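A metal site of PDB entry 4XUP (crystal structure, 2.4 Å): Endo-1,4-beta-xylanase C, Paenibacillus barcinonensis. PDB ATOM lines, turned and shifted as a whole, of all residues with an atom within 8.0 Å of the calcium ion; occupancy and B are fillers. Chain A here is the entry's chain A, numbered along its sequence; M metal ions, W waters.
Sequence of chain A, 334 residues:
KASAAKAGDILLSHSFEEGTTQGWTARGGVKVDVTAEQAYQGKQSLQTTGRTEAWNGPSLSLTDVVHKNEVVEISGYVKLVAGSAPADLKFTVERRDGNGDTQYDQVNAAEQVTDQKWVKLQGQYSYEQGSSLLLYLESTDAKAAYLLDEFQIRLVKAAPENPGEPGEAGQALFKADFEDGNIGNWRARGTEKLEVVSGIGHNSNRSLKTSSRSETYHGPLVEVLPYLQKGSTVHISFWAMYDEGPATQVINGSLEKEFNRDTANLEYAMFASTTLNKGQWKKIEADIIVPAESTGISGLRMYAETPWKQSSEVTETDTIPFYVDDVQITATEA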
ATOM      1  N   HIS A  14       6.997  17.583  15.439  1.00  0.00           N
ATOM      2  CA  HIS A  14       5.794  18.343  15.848  1.00  0.00           C
ATOM      3  C   HIS A  14       5.134  17.727  17.053  1.00  0.00           C
ATOM      4  O   HIS A  14       4.596  16.634  16.958  1.00  0.00           O
ATOM      5  CB  HIS A  14       4.698  18.403  14.775  1.00  0.00           C
ATOM      6  CG  HIS A  14       5.124  19.108  13.538  1.00  0.00           C
ATOM      7  ND1 HIS A  14       4.461  18.958  12.350  1.00  0.00           N
ATOM      8  CD2 HIS A  14       6.172  19.920  13.300  1.00  0.00           C
ATOM      9  CE1 HIS A  14       5.078  19.659  11.421  1.00  0.00           C
ATOM     10  NE2 HIS A  14       6.111  20.261  11.974  1.00  0.00           N
ATOM     11  N   SER A  15       5.160  18.456  18.142  1.00  0.00           N
ATOM     12  CA  SER A  15       4.480  18.096  19.396  1.00  0.00           C
ATOM     13  C   SER A  15       3.172  18.878  19.655  1.00  0.00           C
ATOM     14  O   SER A  15       2.370  18.528  20.530  1.00  0.00           O
ATOM     15  CB  SER A  15       5.435  18.348  20.526  1.00  0.00           C
ATOM     16  OG  SER A  15       5.748  19.720  20.541  1.00  0.00           O
ATOM     17  N   PHE A  16       2.948  19.898  18.830  1.00  0.00           N
ATOM     18  CA  PHE A  16       1.753  20.756  18.854  1.00  0.00           C
ATOM     19  C   PHE A  16       1.539  21.442  20.187  1.00  0.00           C
ATOM     20  O   PHE A  16       0.405  21.746  20.555  1.00  0.00           O
ATOM     21  CB  PHE A  16       0.510  19.983  18.461  1.00  0.00           C
ATOM     22  CG  PHE A  16       0.641  19.287  17.150  1.00  0.00           C
ATOM     23  CD1 PHE A  16       0.587  20.007  15.977  1.00  0.00           C
ATOM     24  CD2 PHE A  16       0.854  17.927  17.089  1.00  0.00           C
ATOM     25  CE1 PHE A  16       0.717  19.379  14.752  1.00  0.00           C
ATOM     26  CE2 PHE A  16       0.997  17.301  15.874  1.00  0.00           C
ATOM     27  CZ  PHE A  16       0.936  18.028  14.701  1.00  0.00           C
ATOM     28  N   GLU A  17       2.626  21.722  20.894  1.00  0.00           N
ATOM     29  CA  GLU A  17       2.555  22.251  22.262  1.00  0.00           C
ATOM     30  C   GLU A  17       2.361  23.785  22.336  1.00  0.00           C
ATOM     31  O   GLU A  17       2.022  24.313  23.406  1.00  0.00           O
ATOM     32  CB  GLU A  17       3.761  21.831  23.110  1.00  0.00           C
ATOM     33  CG  GLU A  17       3.793  20.327  23.417  1.00  0.00           C
ATOM     34  CD  GLU A  17       2.565  19.792  24.165  1.00  0.00           C
ATOM     35  OE1 GLU A  17       2.165  20.388  25.183  1.00  0.00           O
ATOM     36  OE2 GLU A  17       1.944  18.794  23.706  1.00  0.00           O
ATOM     37  N   GLU A  18       2.543  24.468  21.212  1.00  0.00           N
ATOM     38  CA  GLU A  18       2.525  25.949  21.155  1.00  0.00           C
ATOM     39  C   GLU A  18       1.263  26.549  20.541  1.00  0.00           C
ATOM     40  O   GLU A  18       1.248  27.710  20.168  1.00  0.00           O
ATOM     41  CB  GLU A  18       3.762  26.480  20.448  1.00  0.00           C
ATOM     42  CG  GLU A  18       5.089  25.912  20.930  1.00  0.00           C
ATOM     43  CD  GLU A  18       5.733  24.846  20.021  1.00  0.00           C
ATOM     44  OE1 GLU A  18       5.274  24.618  18.864  1.00  0.00           O
ATOM     45  OE2 GLU A  18       6.724  24.230  20.469  1.00  0.00           O
ATOM     46  N   GLN A  22       1.552  23.975  13.346  1.00  0.00           N
ATOM     47  CA  GLN A  22       2.910  23.746  12.832  1.00  0.00           C
ATOM     48  C   GLN A  22       2.928  23.327  11.349  1.00  0.00           C
ATOM     49  O   GLN A  22       3.725  22.510  10.937  1.00  0.00           O
ATOM     50  CB  GLN A  22       3.628  22.717  13.691  1.00  0.00           C
ATOM     51  CG  GLN A  22       3.643  23.097  15.156  1.00  0.00           C
ATOM     52  CD  GLN A  22       4.560  22.231  16.006  1.00  0.00           C
ATOM     53  OE1 GLN A  22       4.115  21.525  16.923  1.00  0.00           O
ATOM     54  NE2 GLN A  22       5.846  22.295  15.729  1.00  0.00           N
ATOM     55  N   VAL A  34      -5.427  22.617  16.913  1.00  0.00           N
ATOM     56  CA  VAL A  34      -4.820  22.132  18.130  1.00  0.00           C
ATOM     57  C   VAL A  34      -5.879  22.028  19.236  1.00  0.00           C
ATOM     58  O   VAL A  34      -6.704  22.915  19.405  1.00  0.00           O
ATOM     59  CB  VAL A  34      -3.679  23.037  18.598  1.00  0.00           C
ATOM     60  CG1 VAL A  34      -3.170  22.660  19.981  1.00  0.00           C
ATOM     61  CG2 VAL A  34      -2.542  22.950  17.609  1.00  0.00           C
ATOM     62  N   THR A  35      -5.799  20.950  19.985  1.00  0.00           N
ATOM     63  CA  THR A  35      -6.596  20.766  21.213  1.00  0.00           C
ATOM     64  C   THR A  35      -5.715  20.524  22.416  1.00  0.00           C
ATOM     65  O   THR A  35      -4.656  19.916  22.332  1.00  0.00           O
ATOM     66  CB  THR A  35      -7.618  19.614  21.115  1.00  0.00           C
ATOM     67  OG1 THR A  35      -8.342  19.525  22.337  1.00  0.00           O
ATOM     68  CG2 THR A  35      -6.969  18.277  20.858  1.00  0.00           C
ATOM     69  N   GLN A  38      -6.795  16.454  25.022  1.00  0.00           N
ATOM     70  CA  GLN A  38      -6.065  15.182  25.012  1.00  0.00           C
ATOM     71  C   GLN A  38      -4.715  15.300  24.302  1.00  0.00           C
ATOM     72  O   GLN A  38      -4.539  16.099  23.403  1.00  0.00           O
ATOM     73  CB  GLN A  38      -6.853  14.071  24.299  1.00  0.00           C
ATOM     74  CG  GLN A  38      -8.142  13.718  24.999  1.00  0.00           C
ATOM     75  CD  GLN A  38      -8.543  12.290  24.797  1.00  0.00           C
ATOM     76  OE1 GLN A  38      -8.386  11.735  23.709  1.00  0.00           O
ATOM     77  NE2 GLN A  38      -9.097  11.659  25.832  1.00  0.00           N
ATOM     78  N   ALA A  39      -3.829  14.394  24.664  1.00  0.00           N
ATOM     79  CA  ALA A  39      -2.464  14.373  24.140  1.00  0.00           C
ATOM     80  C   ALA A  39      -1.726  13.072  24.431  1.00  0.00           C
ATOM     81  O   ALA A  39      -2.037  12.377  25.357  1.00  0.00           O
ATOM     82  CB  ALA A  39      -1.659  15.550  24.700  1.00  0.00           C
ATOM     83  N   TYR A  40      -0.754  12.754  23.595  1.00  0.00           N
ATOM     84  CA  TYR A  40       0.147  11.616  23.827  1.00  0.00           C
ATOM     85  C   TYR A  40       1.267  12.045  24.727  1.00  0.00           C
ATOM     86  O   TYR A  40       1.607  11.398  25.713  1.00  0.00           O
ATOM     87  CB  TYR A  40       0.761  11.093  22.522  1.00  0.00           C
ATOM     88  CG  TYR A  40       1.645   9.866  22.729  1.00  0.00           C
ATOM     89  CD1 TYR A  40       1.093   8.691  23.238  1.00  0.00           C
ATOM     90  CD2 TYR A  40       3.015   9.891  22.433  1.00  0.00           C
ATOM     91  CE1 TYR A  40       1.876   7.579  23.440  1.00  0.00           C
ATOM     92  CE2 TYR A  40       3.812   8.780  22.635  1.00  0.00           C
ATOM     93  CZ  TYR A  40       3.235   7.624  23.154  1.00  0.00           C
ATOM     94  OH  TYR A  40       3.974   6.468  23.318  1.00  0.00           O
ATOM     95  N   GLN A  41       1.852  13.151  24.341  1.00  0.00           N
ATOM     96  CA  GLN A  41       2.934  13.789  25.092  1.00  0.00           C
ATOM     97  C   GLN A  41       2.567  15.246  25.260  1.00  0.00           C
ATOM     98  O   GLN A  41       2.023  15.874  24.327  1.00  0.00           O
ATOM     99  CB  GLN A  41       4.266  13.717  24.340  1.00  0.00           C
ATOM    100  CG  GLN A  41       5.481  13.661  25.291  1.00  0.00           C
ATOM    101  CD  GLN A  41       5.830  12.267  25.821  1.00  0.00           C
ATOM    102  OE1 GLN A  41       5.489  11.237  25.220  1.00  0.00           O
ATOM    103  NE2 GLN A  41       6.553  12.229  26.926  1.00  0.00           N
ATOM    104  N   GLY A  42       2.914  15.773  26.414  1.00  0.00           N
ATOM    105  CA  GLY A  42       2.618  17.148  26.766  1.00  0.00           C
ATOM    106  C   GLY A  42       1.130  17.361  26.992  1.00  0.00           C
ATOM    107  O   GLY A  42       0.396  16.436  27.261  1.00  0.00           O
ATOM    108  N   LYS A  43       0.708  18.603  26.830  1.00  0.00           N
ATOM    109  CA  LYS A  43      -0.700  19.005  27.037  1.00  0.00           C
ATOM    110  C   LYS A  43      -1.590  19.001  25.805  1.00  0.00           C
ATOM    111  O   LYS A  43      -2.801  19.047  25.916  1.00  0.00           O
ATOM    112  CB  LYS A  43      -0.767  20.407  27.605  1.00  0.00           C
ATOM    113  CG  LYS A  43       0.046  20.459  28.876  1.00  0.00           C
ATOM    114  CD  LYS A  43       0.155  21.782  29.546  1.00  0.00           C
ATOM    115  CE  LYS A  43       0.966  21.534  30.820  1.00  0.00           C
ATOM    116  NZ  LYS A  43       2.394  21.820  30.602  1.00  0.00           N
ATOM    117  N   GLN A  44      -0.952  18.995  24.647  1.00  0.00           N
ATOM    118  CA  GLN A  44      -1.671  19.249  23.392  1.00  0.00           C
ATOM    119  C   GLN A  44      -1.367  18.291  22.241  1.00  0.00           C
ATOM    120  O   GLN A  44      -0.307  17.682  22.167  1.00  0.00           O
ATOM    121  CB  GLN A  44      -1.461  20.686  22.905  1.00  0.00           C
ATOM    122  CG  GLN A  44      -1.996  21.746  23.854  1.00  0.00           C
ATOM    123  CD  GLN A  44      -1.762  23.166  23.387  1.00  0.00           C
ATOM    124  OE1 GLN A  44      -0.977  23.428  22.506  1.00  0.00           O
ATOM    125  NE2 GLN A  44      -2.448  24.084  23.994  1.00  0.00           N
ATOM    126  N   SER A  45      -2.360  18.196  21.384  1.00  0.00           N
ATOM    127  CA  SER A  45      -2.287  17.409  20.158  1.00  0.00           C
ATOM    128  C   SER A  45      -3.087  18.057  19.016  1.00  0.00           C
ATOM    129  O   SER A  45      -3.829  19.022  19.210  1.00  0.00           O
ATOM    130  CB  SER A  45      -2.796  15.986  20.407  1.00  0.00           C
ATOM    131  OG  SER A  45      -4.164  16.014  20.750  1.00  0.00           O
ATOM    132  N   LEU A  46      -2.928  17.485  17.838  1.00  0.00           N
ATOM    133  CA  LEU A  46      -3.601  17.933  16.624  1.00  0.00           C
ATOM    134  C   LEU A  46      -4.905  17.198  16.330  1.00  0.00           C
ATOM    135  O   LEU A  46      -4.945  15.996  16.074  1.00  0.00           O
ATOM    136  CB  LEU A  46      -2.690  17.804  15.399  1.00  0.00           C
ATOM    137  CG  LEU A  46      -3.300  18.401  14.117  1.00  0.00           C
ATOM    138  CD1 LEU A  46      -3.307  19.931  14.179  1.00  0.00           C
ATOM    139  CD2 LEU A  46      -2.525  17.960  12.888  1.00  0.00           C
ATOM    140  N   TRP A 118      -3.801   5.543  22.439  1.00  0.00           N
ATOM    141  CA  TRP A 118      -2.907   6.028  21.407  1.00  0.00           C
ATOM    142  C   TRP A 118      -2.175   4.868  20.691  1.00  0.00           C
ATOM    143  O   TRP A 118      -1.783   3.899  21.321  1.00  0.00           O
ATOM    144  CB  TRP A 118      -1.871   6.979  21.944  1.00  0.00           C
ATOM    145  CG  TRP A 118      -2.466   8.260  22.403  1.00  0.00           C
ATOM    146  CD1 TRP A 118      -2.946   8.527  23.637  1.00  0.00           C
ATOM    147  CD2 TRP A 118      -2.663   9.450  21.631  1.00  0.00           C
ATOM    148  NE1 TRP A 118      -3.426   9.799  23.685  1.00  0.00           N
ATOM    149  CE2 TRP A 118      -3.276  10.388  22.466  1.00  0.00           C
ATOM    150  CE3 TRP A 118      -2.404   9.798  20.291  1.00  0.00           C
ATOM    151  CZ2 TRP A 118      -3.617  11.680  22.041  1.00  0.00           C
ATOM    152  CZ3 TRP A 118      -2.764  11.080  19.857  1.00  0.00           C
ATOM    153  CH2 TRP A 118      -3.348  12.010  20.742  1.00  0.00           C
ATOM    154  N   LEU A 148      -3.760  13.514  16.384  1.00  0.00           N
ATOM    155  CA  LEU A 148      -2.377  13.223  16.002  1.00  0.00           C
ATOM    156  C   LEU A 148      -1.463  13.959  16.921  1.00  0.00           C
ATOM    157  O   LEU A 148      -1.648  15.130  17.150  1.00  0.00           O
ATOM    158  CB  LEU A 148      -2.067  13.652  14.548  1.00  0.00           C
ATOM    159  CG  LEU A 148      -0.594  13.578  14.126  1.00  0.00           C
ATOM    160  CD1 LEU A 148      -0.108  12.149  14.065  1.00  0.00           C
ATOM    161  CD2 LEU A 148      -0.424  14.205  12.725  1.00  0.00           C
ATOM    162  N   ASP A 149      -0.427  13.271  17.381  1.00  0.00           N
ATOM    163  CA  ASP A 149       0.570  13.867  18.255  1.00  0.00           C
ATOM    164  C   ASP A 149       1.942  13.253  18.039  1.00  0.00           C
ATOM    165  O   ASP A 149       2.061  12.203  17.494  1.00  0.00           O
ATOM    166  CB  ASP A 149       0.141  13.730  19.717  1.00  0.00           C
ATOM    167  CG  ASP A 149       0.761  14.789  20.604  1.00  0.00           C
ATOM    168  OD1 ASP A 149       1.513  15.649  20.097  1.00  0.00           O
ATOM    169  OD2 ASP A 149       0.551  14.750  21.840  1.00  0.00           O
ATOM    170  N   GLU A 150       2.959  13.963  18.507  1.00  0.00           N
ATOM    171  CA  GLU A 150       4.361  13.558  18.420  1.00  0.00           C
ATOM    172  C   GLU A 150       4.688  13.036  17.039  1.00  0.00           C
ATOM    173  O   GLU A 150       5.121  11.929  16.834  1.00  0.00           O
ATOM    174  CB  GLU A 150       4.712  12.531  19.474  1.00  0.00           C
ATOM    175  CG  GLU A 150       4.787  13.137  20.867  1.00  0.00           C
ATOM    176  CD  GLU A 150       5.780  14.301  20.995  1.00  0.00           C
ATOM    177  OE1 GLU A 150       7.006  14.092  20.892  1.00  0.00           O
ATOM    178  OE2 GLU A 150       5.313  15.445  21.179  1.00  0.00           O
ATOM    179  N   PHE A 151       4.392  13.889  16.083  1.00  0.00           N
ATOM    180  CA  PHE A 151       4.630  13.596  14.682  1.00  0.00           C
ATOM    181  C   PHE A 151       6.071  13.881  14.394  1.00  0.00           C
ATOM    182  O   PHE A 151       6.634  14.884  14.813  1.00  0.00           O
ATOM    183  CB  PHE A 151       3.752  14.429  13.752  1.00  0.00           C
ATOM    184  CG  PHE A 151       4.098  14.277  12.294  1.00  0.00           C
ATOM    185  CD1 PHE A 151       3.688  13.168  11.577  1.00  0.00           C
ATOM    186  CD2 PHE A 151       4.858  15.225  11.653  1.00  0.00           C
ATOM    187  CE1 PHE A 151       4.000  13.024  10.239  1.00  0.00           C
ATOM    188  CE2 PHE A 151       5.198  15.084  10.314  1.00  0.00           C
ATOM    189  CZ  PHE A 151       4.775  13.960   9.609  1.00  0.00           C
HETATM  190 CA    CA M   1       1.725  16.872  22.253  1.00  0.00          CA
HETATM  191  O   HOH W   1       3.655  16.483  22.671  1.00  0.00           O
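The calcium ion is bound by water W1 (2.0 Å), the backbone carbonyl oxygen (O) of Gln 44 (2.2 Å), the backbone carbonyl oxygen (O) of Gln 41 (2.3 Å), the side-chain carboxylate (OE2) of Glu 17 (2.4 Å), the side-chain carboxylate (OD2) of Asp 149 (2.5 Å), the backbone carbonyl oxygen (O) of Ser 15 (2.5 Å) and the side-chain carboxylate (OD1) of Asp 149 (2.5 Å). The calcium ion has seven donor atoms within binding distance.
Within 4 Å of the calcium ion: Ser 15, Glu 17, Gln 41, Gln 44 and Asp 149. The nearest printed residue that does not touch the calcium ion is Glu 150 (4.01 Å).
O of Phe 16 lies close to OE1 of Gln 44 (2.9 Å). N of Tyr 40 sits close to OD2 of Asp 149 (3.0 Å). The backbone NH (N) of Ser 15 lies within hydrogen-bond range of the side-chain amide oxygen (OE1) of Gln 22 (3.5 Å). The backbone NH (N) of Lys 43 is in hydrogen-bond range of the side-chain carboxylate (OE1) of Glu 17, at 2.8 Å.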
